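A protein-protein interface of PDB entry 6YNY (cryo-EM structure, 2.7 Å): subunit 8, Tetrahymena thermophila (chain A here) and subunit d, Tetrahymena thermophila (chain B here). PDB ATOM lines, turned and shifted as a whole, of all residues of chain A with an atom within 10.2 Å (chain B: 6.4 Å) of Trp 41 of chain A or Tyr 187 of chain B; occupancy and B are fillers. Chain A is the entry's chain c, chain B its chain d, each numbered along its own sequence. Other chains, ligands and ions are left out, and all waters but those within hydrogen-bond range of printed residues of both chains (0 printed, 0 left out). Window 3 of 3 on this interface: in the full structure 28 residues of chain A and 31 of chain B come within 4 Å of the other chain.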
ATOM      1  N   TYR A  33      29.199  24.025   9.083  1.00  0.00           N
ATOM      2  CA  TYR A  33      27.922  23.804   8.419  1.00  0.00           C
ATOM      3  C   TYR A  33      28.114  23.151   7.058  1.00  0.00           C
ATOM      4  O   TYR A  33      27.332  22.277   6.667  1.00  0.00           O
ATOM      5  CB  TYR A  33      27.183  25.135   8.288  1.00  0.00           C
ATOM      6  CG  TYR A  33      25.732  25.015   7.909  1.00  0.00           C
ATOM      7  CD1 TYR A  33      24.809  24.502   8.798  1.00  0.00           C
ATOM      8  CD2 TYR A  33      25.284  25.434   6.669  1.00  0.00           C
ATOM      9  CE1 TYR A  33      23.486  24.395   8.463  1.00  0.00           C
ATOM     10  CE2 TYR A  33      23.958  25.329   6.323  1.00  0.00           C
ATOM     11  CZ  TYR A  33      23.062  24.810   7.225  1.00  0.00           C
ATOM     12  OH  TYR A  33      21.738  24.705   6.886  1.00  0.00           O
ATOM     13  N   CYS A  34      29.151  23.556   6.324  1.00  0.00           N
ATOM     14  CA  CYS A  34      29.425  22.933   5.034  1.00  0.00           C
ATOM     15  C   CYS A  34      29.842  21.481   5.211  1.00  0.00           C
ATOM     16  O   CYS A  34      29.354  20.594   4.503  1.00  0.00           O
ATOM     17  CB  CYS A  34      30.512  23.713   4.295  1.00  0.00           C
ATOM     18  SG  CYS A  34      30.718  23.228   2.571  1.00  0.00           S
ATOM     19  N   THR A  35      30.745  21.220   6.156  1.00  0.00           N
ATOM     20  CA  THR A  35      31.157  19.849   6.424  1.00  0.00           C
ATOM     21  C   THR A  35      29.963  18.974   6.774  1.00  0.00           C
ATOM     22  O   THR A  35      29.854  17.840   6.298  1.00  0.00           O
ATOM     23  CB  THR A  35      32.182  19.830   7.555  1.00  0.00           C
ATOM     24  OG1 THR A  35      33.311  20.631   7.193  1.00  0.00           O
ATOM     25  CG2 THR A  35      32.641  18.423   7.843  1.00  0.00           C
ATOM     26  N   MET A  36      29.055  19.485   7.605  1.00  0.00           N
ATOM     27  CA  MET A  36      27.880  18.714   7.987  1.00  0.00           C
ATOM     28  C   MET A  36      27.006  18.404   6.779  1.00  0.00           C
ATOM     29  O   MET A  36      26.613  17.253   6.562  1.00  0.00           O
ATOM     30  CB  MET A  36      27.089  19.474   9.049  1.00  0.00           C
ATOM     31  CG  MET A  36      25.925  18.703   9.630  1.00  0.00           C
ATOM     32  SD  MET A  36      24.434  18.753   8.624  1.00  0.00           S
ATOM     33  CE  MET A  36      23.873  20.414   8.961  1.00  0.00           C
ATOM     34  N   ASN A  37      26.687  19.424   5.979  1.00  0.00           N
ATOM     35  CA  ASN A  37      25.848  19.204   4.808  1.00  0.00           C
ATOM     36  C   ASN A  37      26.533  18.306   3.790  1.00  0.00           C
ATOM     37  O   ASN A  37      25.863  17.560   3.070  1.00  0.00           O
ATOM     38  CB  ASN A  37      25.473  20.543   4.179  1.00  0.00           C
ATOM     39  CG  ASN A  37      24.452  21.300   4.994  1.00  0.00           C
ATOM     40  OD1 ASN A  37      23.250  21.120   4.822  1.00  0.00           O
ATOM     41  ND2 ASN A  37      24.925  22.154   5.886  1.00  0.00           N
ATOM     42  N   PHE A  38      27.862  18.362   3.718  1.00  0.00           N
ATOM     43  CA  PHE A  38      28.593  17.475   2.822  1.00  0.00           C
ATOM     44  C   PHE A  38      28.379  16.016   3.196  1.00  0.00           C
ATOM     45  O   PHE A  38      28.174  15.166   2.322  1.00  0.00           O
ATOM     46  CB  PHE A  38      30.075  17.844   2.846  1.00  0.00           C
ATOM     47  CG  PHE A  38      30.991  16.749   2.403  1.00  0.00           C
ATOM     48  CD1 PHE A  38      30.852  16.159   1.165  1.00  0.00           C
ATOM     49  CD2 PHE A  38      32.018  16.329   3.221  1.00  0.00           C
ATOM     50  CE1 PHE A  38      31.702  15.158   0.765  1.00  0.00           C
ATOM     51  CE2 PHE A  38      32.872  15.331   2.821  1.00  0.00           C
ATOM     52  CZ  PHE A  38      32.716  14.748   1.591  1.00  0.00           C
ATOM     53  N   LEU A  39      28.413  15.708   4.491  1.00  0.00           N
ATOM     54  CA  LEU A  39      28.209  14.333   4.929  1.00  0.00           C
ATOM     55  C   LEU A  39      26.775  13.888   4.693  1.00  0.00           C
ATOM     56  O   LEU A  39      26.530  12.757   4.258  1.00  0.00           O
ATOM     57  CB  LEU A  39      28.562  14.204   6.406  1.00  0.00           C
ATOM     58  CG  LEU A  39      29.985  14.591   6.798  1.00  0.00           C
ATOM     59  CD1 LEU A  39      30.157  14.556   8.299  1.00  0.00           C
ATOM     60  CD2 LEU A  39      30.977  13.678   6.134  1.00  0.00           C
ATOM     61  N   ALA A  40      25.813  14.764   4.976  1.00  0.00           N
ATOM     62  CA  ALA A  40      24.409  14.400   4.856  1.00  0.00           C
ATOM     63  C   ALA A  40      23.988  14.281   3.398  1.00  0.00           C
ATOM     64  O   ALA A  40      23.406  13.271   2.990  1.00  0.00           O
ATOM     65  CB  ALA A  40      23.554  15.431   5.580  1.00  0.00           C
ATOM     66  N   TRP A  41      24.276  15.303   2.593  1.00  0.00           N
ATOM     67  CA  TRP A  41      23.822  15.300   1.208  1.00  0.00           C
ATOM     68  C   TRP A  41      24.518  14.218   0.396  1.00  0.00           C
ATOM     69  O   TRP A  41      23.880  13.546  -0.422  1.00  0.00           O
ATOM     70  CB  TRP A  41      24.048  16.671   0.581  1.00  0.00           C
ATOM     71  CG  TRP A  41      23.025  17.672   0.981  1.00  0.00           C
ATOM     72  CD1 TRP A  41      23.127  18.596   1.970  1.00  0.00           C
ATOM     73  CD2 TRP A  41      21.731  17.845   0.401  1.00  0.00           C
ATOM     74  NE1 TRP A  41      21.980  19.339   2.043  1.00  0.00           N
ATOM     75  CE2 TRP A  41      21.105  18.897   1.089  1.00  0.00           C
ATOM     76  CE3 TRP A  41      21.040  17.212  -0.633  1.00  0.00           C
ATOM     77  CZ2 TRP A  41      19.824  19.331   0.776  1.00  0.00           C
ATOM     78  CZ3 TRP A  41      19.772  17.643  -0.942  1.00  0.00           C
ATOM     79  CH2 TRP A  41      19.176  18.692  -0.241  1.00  0.00           C
ATOM     80  N   SER A  42      25.821  14.033   0.601  1.00  0.00           N
ATOM     81  CA  SER A  42      26.529  12.981  -0.118  1.00  0.00           C
ATOM     82  C   SER A  42      25.933  11.615   0.189  1.00  0.00           C
ATOM     83  O   SER A  42      25.870  10.746  -0.685  1.00  0.00           O
ATOM     84  CB  SER A  42      28.016  13.009   0.233  1.00  0.00           C
ATOM     85  OG  SER A  42      28.219  12.844   1.620  1.00  0.00           O
ATOM     86  N   THR A  43      25.476  11.413   1.424  1.00  0.00           N
ATOM     87  CA  THR A  43      24.885  10.133   1.791  1.00  0.00           C
ATOM     88  C   THR A  43      23.551   9.920   1.089  1.00  0.00           C
ATOM     89  O   THR A  43      23.211   8.793   0.717  1.00  0.00           O
ATOM     90  CB  THR A  43      24.705  10.056   3.306  1.00  0.00           C
ATOM     91  OG1 THR A  43      25.978  10.165   3.950  1.00  0.00           O
ATOM     92  CG2 THR A  43      24.052   8.755   3.704  1.00  0.00           C
ATOM     93  N   VAL A  44      22.785  10.992   0.896  1.00  0.00           N
ATOM     94  CA  VAL A  44      21.459  10.866   0.304  1.00  0.00           C
ATOM     95  C   VAL A  44      21.560  10.600  -1.191  1.00  0.00           C
ATOM     96  O   VAL A  44      20.950   9.659  -1.713  1.00  0.00           O
ATOM     97  CB  VAL A  44      20.633  12.130   0.593  1.00  0.00           C
ATOM     98  CG1 VAL A  44      19.340  12.107  -0.179  1.00  0.00           C
ATOM     99  CG2 VAL A  44      20.364  12.246   2.071  1.00  0.00           C
ATOM    100  N   VAL A  45      22.329  11.421  -1.902  1.00  0.00           N
ATOM    101  CA  VAL A  45      22.356  11.334  -3.355  1.00  0.00           C
ATOM    102  C   VAL A  45      23.158  10.127  -3.824  1.00  0.00           C
ATOM    103  O   VAL A  45      22.918   9.610  -4.920  1.00  0.00           O
ATOM    104  CB  VAL A  45      22.905  12.643  -3.943  1.00  0.00           C
ATOM    105  CG1 VAL A  45      22.926  12.582  -5.459  1.00  0.00           C
ATOM    106  CG2 VAL A  45      22.069  13.813  -3.464  1.00  0.00           C
ATOM    107  N   GLU A  46      24.113   9.660  -3.023  1.00  0.00           N
ATOM    108  CA  GLU A  46      24.899   8.495  -3.408  1.00  0.00           C
ATOM    109  C   GLU A  46      24.143   7.195  -3.183  1.00  0.00           C
ATOM    110  O   GLU A  46      24.292   6.255  -3.968  1.00  0.00           O
ATOM    111  CB  GLU A  46      26.215   8.456  -2.630  1.00  0.00           C
ATOM    112  CG  GLU A  46      27.204   9.536  -3.021  1.00  0.00           C
ATOM    113  CD  GLU A  46      28.509   9.434  -2.256  1.00  0.00           C
ATOM    114  OE1 GLU A  46      28.907   8.307  -1.901  1.00  0.00           O
ATOM    115  OE2 GLU A  46      29.132  10.484  -2.000  1.00  0.00           O
ATOM    116  N   LEU A  47      23.325   7.127  -2.136  1.00  0.00           N
ATOM    117  CA  LEU A  47      22.699   5.883  -1.715  1.00  0.00           C
ATOM    118  C   LEU A  47      21.407   5.576  -2.458  1.00  0.00           C
ATOM    119  O   LEU A  47      20.575   4.820  -1.947  1.00  0.00           O
ATOM    120  CB  LEU A  47      22.449   5.907  -0.210  1.00  0.00           C
ATOM    121  CG  LEU A  47      23.693   5.625   0.627  1.00  0.00           C
ATOM    122  CD1 LEU A  47      23.390   5.760   2.087  1.00  0.00           C
ATOM    123  CD2 LEU A  47      24.219   4.243   0.329  1.00  0.00           C
ATOM    124  N   ILE A  48      21.214   6.148  -3.646  1.00  0.00           N
ATOM    125  CA  ILE A  48      20.141   5.680  -4.518  1.00  0.00           C
ATOM    126  C   ILE A  48      20.565   4.484  -5.350  1.00  0.00           C
ATOM    127  O   ILE A  48      19.714   3.851  -5.985  1.00  0.00           O
ATOM    128  CB  ILE A  48      19.655   6.794  -5.462  1.00  0.00           C
ATOM    129  CG1 ILE A  48      20.788   7.270  -6.366  1.00  0.00           C
ATOM    130  CG2 ILE A  48      19.109   7.951  -4.665  1.00  0.00           C
ATOM    131  CD1 ILE A  48      20.375   8.323  -7.340  1.00  0.00           C
ATOM    132  N   TRP A  49      21.851   4.149  -5.355  1.00  0.00           N
ATOM    133  CA  TRP A  49      22.373   3.113  -6.233  1.00  0.00           C
ATOM    134  C   TRP A  49      22.005   1.707  -5.770  1.00  0.00           C
ATOM    135  O   TRP A  49      21.788   0.832  -6.616  1.00  0.00           O
ATOM    136  CB  TRP A  49      23.891   3.260  -6.382  1.00  0.00           C
ATOM    137  CG  TRP A  49      24.737   2.730  -5.269  1.00  0.00           C
ATOM    138  CD1 TRP A  49      25.345   3.454  -4.292  1.00  0.00           C
ATOM    139  CD2 TRP A  49      25.093   1.365  -5.033  1.00  0.00           C
ATOM    140  NE1 TRP A  49      26.049   2.630  -3.458  1.00  0.00           N
ATOM    141  CE2 TRP A  49      25.909   1.339  -3.891  1.00  0.00           C
ATOM    142  CE3 TRP A  49      24.796   0.163  -5.674  1.00  0.00           C
ATOM    143  CZ2 TRP A  49      26.428   0.163  -3.377  1.00  0.00           C
ATOM    144  CZ3 TRP A  49      25.311  -0.999  -5.163  1.00  0.00           C
ATOM    145  CH2 TRP A  49      26.117  -0.995  -4.029  1.00  0.00           C
ATOM    146  N   PRO A  50      21.921   1.426  -4.466  1.00  0.00           N
ATOM    147  CA  PRO A  50      21.514   0.070  -4.072  1.00  0.00           C
ATOM    148  C   PRO A  50      20.105  -0.265  -4.520  1.00  0.00           C
ATOM    149  O   PRO A  50      19.837  -1.396  -4.941  1.00  0.00           O
ATOM    150  CB  PRO A  50      21.650   0.092  -2.545  1.00  0.00           C
ATOM    151  CG  PRO A  50      22.463   1.275  -2.234  1.00  0.00           C
ATOM    152  CD  PRO A  50      22.137   2.267  -3.279  1.00  0.00           C
ATOM    153  N   THR A  51      19.195   0.705  -4.446  1.00  0.00           N
ATOM    154  CA  THR A  51      17.828   0.487  -4.898  1.00  0.00           C
ATOM    155  C   THR A  51      17.767   0.337  -6.411  1.00  0.00           C
ATOM    156  O   THR A  51      17.036  -0.515  -6.929  1.00  0.00           O
ATOM    157  CB  THR A  51      16.946   1.646  -4.436  1.00  0.00           C
ATOM    158  OG1 THR A  51      16.838   1.634  -3.011  1.00  0.00           O
ATOM    159  CG2 THR A  51      15.574   1.556  -5.045  1.00  0.00           C
ATOM    160  N   HIS A  52      18.526   1.157  -7.134  1.00  0.00           N
ATOM    161  CA  HIS A  52      18.543   1.065  -8.587  1.00  0.00           C
ATOM    162  C   HIS A  52      19.161  -0.247  -9.050  1.00  0.00           C
ATOM    163  O   HIS A  52      18.707  -0.845 -10.030  1.00  0.00           O
ATOM    164  CB  HIS A  52      19.307   2.254  -9.162  1.00  0.00           C
ATOM    165  CG  HIS A  52      19.285   2.326 -10.652  1.00  0.00           C
ATOM    166  ND1 HIS A  52      20.379   2.016 -11.427  1.00  0.00           N
ATOM    167  CD2 HIS A  52      18.301   2.677 -11.513  1.00  0.00           C
ATOM    168  CE1 HIS A  52      20.072   2.171 -12.700  1.00  0.00           C
ATOM    169  NE2 HIS A  52      18.816   2.571 -12.780  1.00  0.00           N
ATOM    170  N   LEU B 181      19.791   9.885 -13.143  1.00  0.00           N
ATOM    171  CA  LEU B 181      19.040  10.210 -11.936  1.00  0.00           C
ATOM    172  C   LEU B 181      19.747  11.287 -11.128  1.00  0.00           C
ATOM    173  O   LEU B 181      19.105  12.201 -10.600  1.00  0.00           O
ATOM    174  CB  LEU B 181      18.846   8.956 -11.090  1.00  0.00           C
ATOM    175  CG  LEU B 181      18.163   7.774 -11.767  1.00  0.00           C
ATOM    176  CD1 LEU B 181      18.242   6.558 -10.878  1.00  0.00           C
ATOM    177  CD2 LEU B 181      16.728   8.101 -12.101  1.00  0.00           C
ATOM    178  N   THR B 182      21.071  11.197 -11.026  1.00  0.00           N
ATOM    179  CA  THR B 182      21.822  12.158 -10.230  1.00  0.00           C
ATOM    180  C   THR B 182      21.835  13.531 -10.888  1.00  0.00           C
ATOM    181  O   THR B 182      21.646  14.549 -10.214  1.00  0.00           O
ATOM    182  CB  THR B 182      23.246  11.648 -10.019  1.00  0.00           C
ATOM    183  OG1 THR B 182      23.206  10.336  -9.444  1.00  0.00           O
ATOM    184  CG2 THR B 182      24.015  12.562  -9.107  1.00  0.00           C
ATOM    185  N   THR B 184      19.671  14.804 -12.928  1.00  0.00           N
ATOM    186  CA  THR B 184      18.338  15.385 -12.881  1.00  0.00           C
ATOM    187  C   THR B 184      17.818  15.541 -11.461  1.00  0.00           C
ATOM    188  O   THR B 184      16.667  15.947 -11.277  1.00  0.00           O
ATOM    189  CB  THR B 184      17.359  14.537 -13.695  1.00  0.00           C
ATOM    190  OG1 THR B 184      17.407  13.176 -13.255  1.00  0.00           O
ATOM    191  CG2 THR B 184      17.705  14.605 -15.157  1.00  0.00           C
ATOM    192  N   HIS B 185      18.641  15.241 -10.461  1.00  0.00           N
ATOM    193  CA  HIS B 185      18.263  15.368  -9.057  1.00  0.00           C
ATOM    194  C   HIS B 185      17.022  14.542  -8.735  1.00  0.00           C
ATOM    195  O   HIS B 185      16.154  14.960  -7.969  1.00  0.00           O
ATOM    196  CB  HIS B 185      18.070  16.833  -8.674  1.00  0.00           C
ATOM    197  CG  HIS B 185      19.343  17.533  -8.325  1.00  0.00           C
ATOM    198  ND1 HIS B 185      19.374  18.696  -7.589  1.00  0.00           N
ATOM    199  CD2 HIS B 185      20.632  17.231  -8.606  1.00  0.00           C
ATOM    200  CE1 HIS B 185      20.627  19.081  -7.433  1.00  0.00           C
ATOM    201  NE2 HIS B 185      21.409  18.210  -8.040  1.00  0.00           N
ATOM    202  N   ASN B 186      16.944  13.353  -9.323  1.00  0.00           N
ATOM    203  CA  ASN B 186      15.951  12.357  -8.933  1.00  0.00           C
ATOM    204  C   ASN B 186      16.554  11.420  -7.889  1.00  0.00           C
ATOM    205  O   ASN B 186      16.645  10.206  -8.062  1.00  0.00           O
ATOM    206  CB  ASN B 186      15.453  11.595 -10.154  1.00  0.00           C
ATOM    207  CG  ASN B 186      14.402  12.353 -10.925  1.00  0.00           C
ATOM    208  OD1 ASN B 186      13.220  12.313 -10.590  1.00  0.00           O
ATOM    209  ND2 ASN B 186      14.822  13.046 -11.969  1.00  0.00           N
ATOM    210  N   TYR B 187      16.982  12.027  -6.784  1.00  0.00           N
ATOM    211  CA  TYR B 187      17.669  11.319  -5.718  1.00  0.00           C
ATOM    212  C   TYR B 187      16.713  10.691  -4.714  1.00  0.00           C
ATOM    213  O   TYR B 187      17.127  10.371  -3.595  1.00  0.00           O
ATOM    214  CB  TYR B 187      18.650  12.252  -5.005  1.00  0.00           C
ATOM    215  CG  TYR B 187      18.059  13.525  -4.452  1.00  0.00           C
ATOM    216  CD1 TYR B 187      18.260  14.736  -5.090  1.00  0.00           C
ATOM    217  CD2 TYR B 187      17.318  13.519  -3.283  1.00  0.00           C
ATOM    218  CE1 TYR B 187      17.737  15.900  -4.587  1.00  0.00           C
ATOM    219  CE2 TYR B 187      16.788  14.680  -2.772  1.00  0.00           C
ATOM    220  CZ  TYR B 187      17.000  15.868  -3.428  1.00  0.00           C
ATOM    221  OH  TYR B 187      16.476  17.032  -2.925  1.00  0.00           O
ATOM    222  N   ILE B 188      15.450  10.510  -5.085  1.00  0.00           N
ATOM    223  CA  ILE B 188      14.509   9.713  -4.304  1.00  0.00           C
ATOM    224  C   ILE B 188      14.562   8.287  -4.849  1.00  0.00           C
ATOM    225  O   ILE B 188      14.181   8.071  -6.011  1.00  0.00           O
ATOM    226  CB  ILE B 188      13.089  10.281  -4.372  1.00  0.00           C
ATOM    227  CG1 ILE B 188      13.072  11.717  -3.855  1.00  0.00           C
ATOM    228  CG2 ILE B 188      12.156   9.422  -3.564  1.00  0.00           C
ATOM    229  CD1 ILE B 188      11.737  12.394  -3.974  1.00  0.00           C
ATOM    230  N   PRO B 189      15.020   7.309  -4.073  1.00  0.00           N
ATOM    231  CA  PRO B 189      15.247   5.975  -4.639  1.00  0.00           C
ATOM    232  C   PRO B 189      13.956   5.316  -5.102  1.00  0.00           C
ATOM    233  O   PRO B 189      12.950   5.304  -4.391  1.00  0.00           O
ATOM    234  CB  PRO B 189      15.897   5.213  -3.481  1.00  0.00           C
ATOM    235  CG  PRO B 189      15.495   5.930  -2.273  1.00  0.00           C
ATOM    236  CD  PRO B 189      15.390   7.364  -2.652  1.00  0.00           C
ATOM    237  N   HIS B 217       9.651  13.906  -8.318  1.00  0.00           N
ATOM    238  CA  HIS B 217      10.878  14.673  -8.181  1.00  0.00           C
ATOM    239  C   HIS B 217      10.911  15.391  -6.838  1.00  0.00           C
ATOM    240  O   HIS B 217       9.883  15.900  -6.383  1.00  0.00           O
ATOM    241  CB  HIS B 217      10.999  15.697  -9.308  1.00  0.00           C
ATOM    242  CG  HIS B 217      12.381  16.235  -9.489  1.00  0.00           C
ATOM    243  ND1 HIS B 217      12.867  17.300  -8.766  1.00  0.00           N
ATOM    244  CD2 HIS B 217      13.382  15.853 -10.315  1.00  0.00           C
ATOM    245  CE1 HIS B 217      14.110  17.549  -9.135  1.00  0.00           C
ATOM    246  NE2 HIS B 217      14.445  16.688 -10.077  1.00  0.00           N
ATOM    247  N   PRO B 218      12.067  15.453  -6.170  1.00  0.00           N
ATOM    248  CA  PRO B 218      12.132  16.120  -4.863  1.00  0.00           C
ATOM    249  C   PRO B 218      11.910  17.621  -4.909  1.00  0.00           C
ATOM    250  O   PRO B 218      11.890  18.254  -3.848  1.00  0.00           O
ATOM    251  CB  PRO B 218      13.549  15.791  -4.376  1.00  0.00           C
ATOM    252  CG  PRO B 218      14.299  15.418  -5.580  1.00  0.00           C
ATOM    253  CD  PRO B 218      13.337  14.797  -6.511  1.00  0.00           C
ATOM    254  N   ALA B 219      11.739  18.212  -6.089  1.00  0.00           N
ATOM    255  CA  ALA B 219      11.554  19.647  -6.220  1.00  0.00           C
ATOM    256  C   ALA B 219      10.151  20.043  -6.642  1.00  0.00           C
ATOM    257  O   ALA B 219       9.776  21.204  -6.460  1.00  0.00           O
ATOM    258  CB  ALA B 219      12.548  20.221  -7.236  1.00  0.00           C
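Hydrophobic or aromatic side chains of chain A that line the printed part of chain B: Trp 41, Val 44, Val 45, Ile 48 and His 52.
Printed residues of chain B that touch a printed residue of chain A: Leu 181, Thr 182, Tyr 187 and Pro 189.
Hydrophobic or aromatic side chains of chain B within 4 Å of the printed part of chain A: Leu 181, Tyr 187 and Pro 189.
Among the printed residues, 6 pairs touch across the chains.
Among the printed residues, no Asp or Glu carboxylate lies within 4 Å of a Lys or Arg side-chain nitrogen of the other chain.
The side-chain hydroxyl (OG1) of Thr 184 of chain B sits at hydrogen-bond distance from the backbone carbonyl oxygen (O) of Leu 181 of chain B, 3.3 Å away.
O of Leu 181 of chain B sits at hydrogen-bond distance from N of Asn 186 of chain B, at 2.8 Å.
Among the printed residues, pairs that only touch across the chains: Trp 41 of chain A with Tyr 187 of chain B (3.9 Å), Val 44 of chain A with Tyr 187 of chain B (3.96 Å), Val 45 of chain A with Thr 182 of chain B (3.8 Å), Ile 48 of chain A with Tyr 187 of chain B (3.3 Å), Thr 51 of chain A with Pro 189 of chain B (3.7 Å) and His 52 of chain A with Leu 181 of chain B (3.9 Å).
Of chain B, only Tyr 187 comes within 4 Å of Trp 41 of chain A.
Of chain A, only Trp 41 (3.9 Å), Val 44 (3.96 Å) and Ile 48 (3.3 Å) come within 4 Å of Tyr 187 of chain B.
His 185 of chain B touches none of the printed residues of chain A.
No residue of chain A comes within 4 Å of Asn 186 of chain B.
No residue of chain A comes within 4 Å of Ile 188 of chain B.
No residue of chain A comes within 4 Å of Pro 218 of chain B.
Printed residues of chain A within 4 Å of Pro 189 of chain B: Thr 51 (3.7 Å).
Of the printed residues of chain B, Ile 48 of chain A touches Tyr 187.
Printed residues of chain A within 4 Å of Leu 181 of chain B: His 52.
Printed residues of chain B within 4 Å of Val 44 of chain A: Tyr 187 (3.96 Å).
Of the printed residues of chain B, Thr 51 of chain A touches Pro 189.
Ala 40 of chain A touches none of the printed residues of chain B.
Phe 38 of chain A touches none of the printed residues of chain B.
The nearest printed residue of chain B that does not touch Trp 41 of chain A is His 185 of chain B (6.7 Å).
The nearest residue of chain A that does not touch Tyr 187 of chain B is Val 45 of chain A (4.1 Å).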
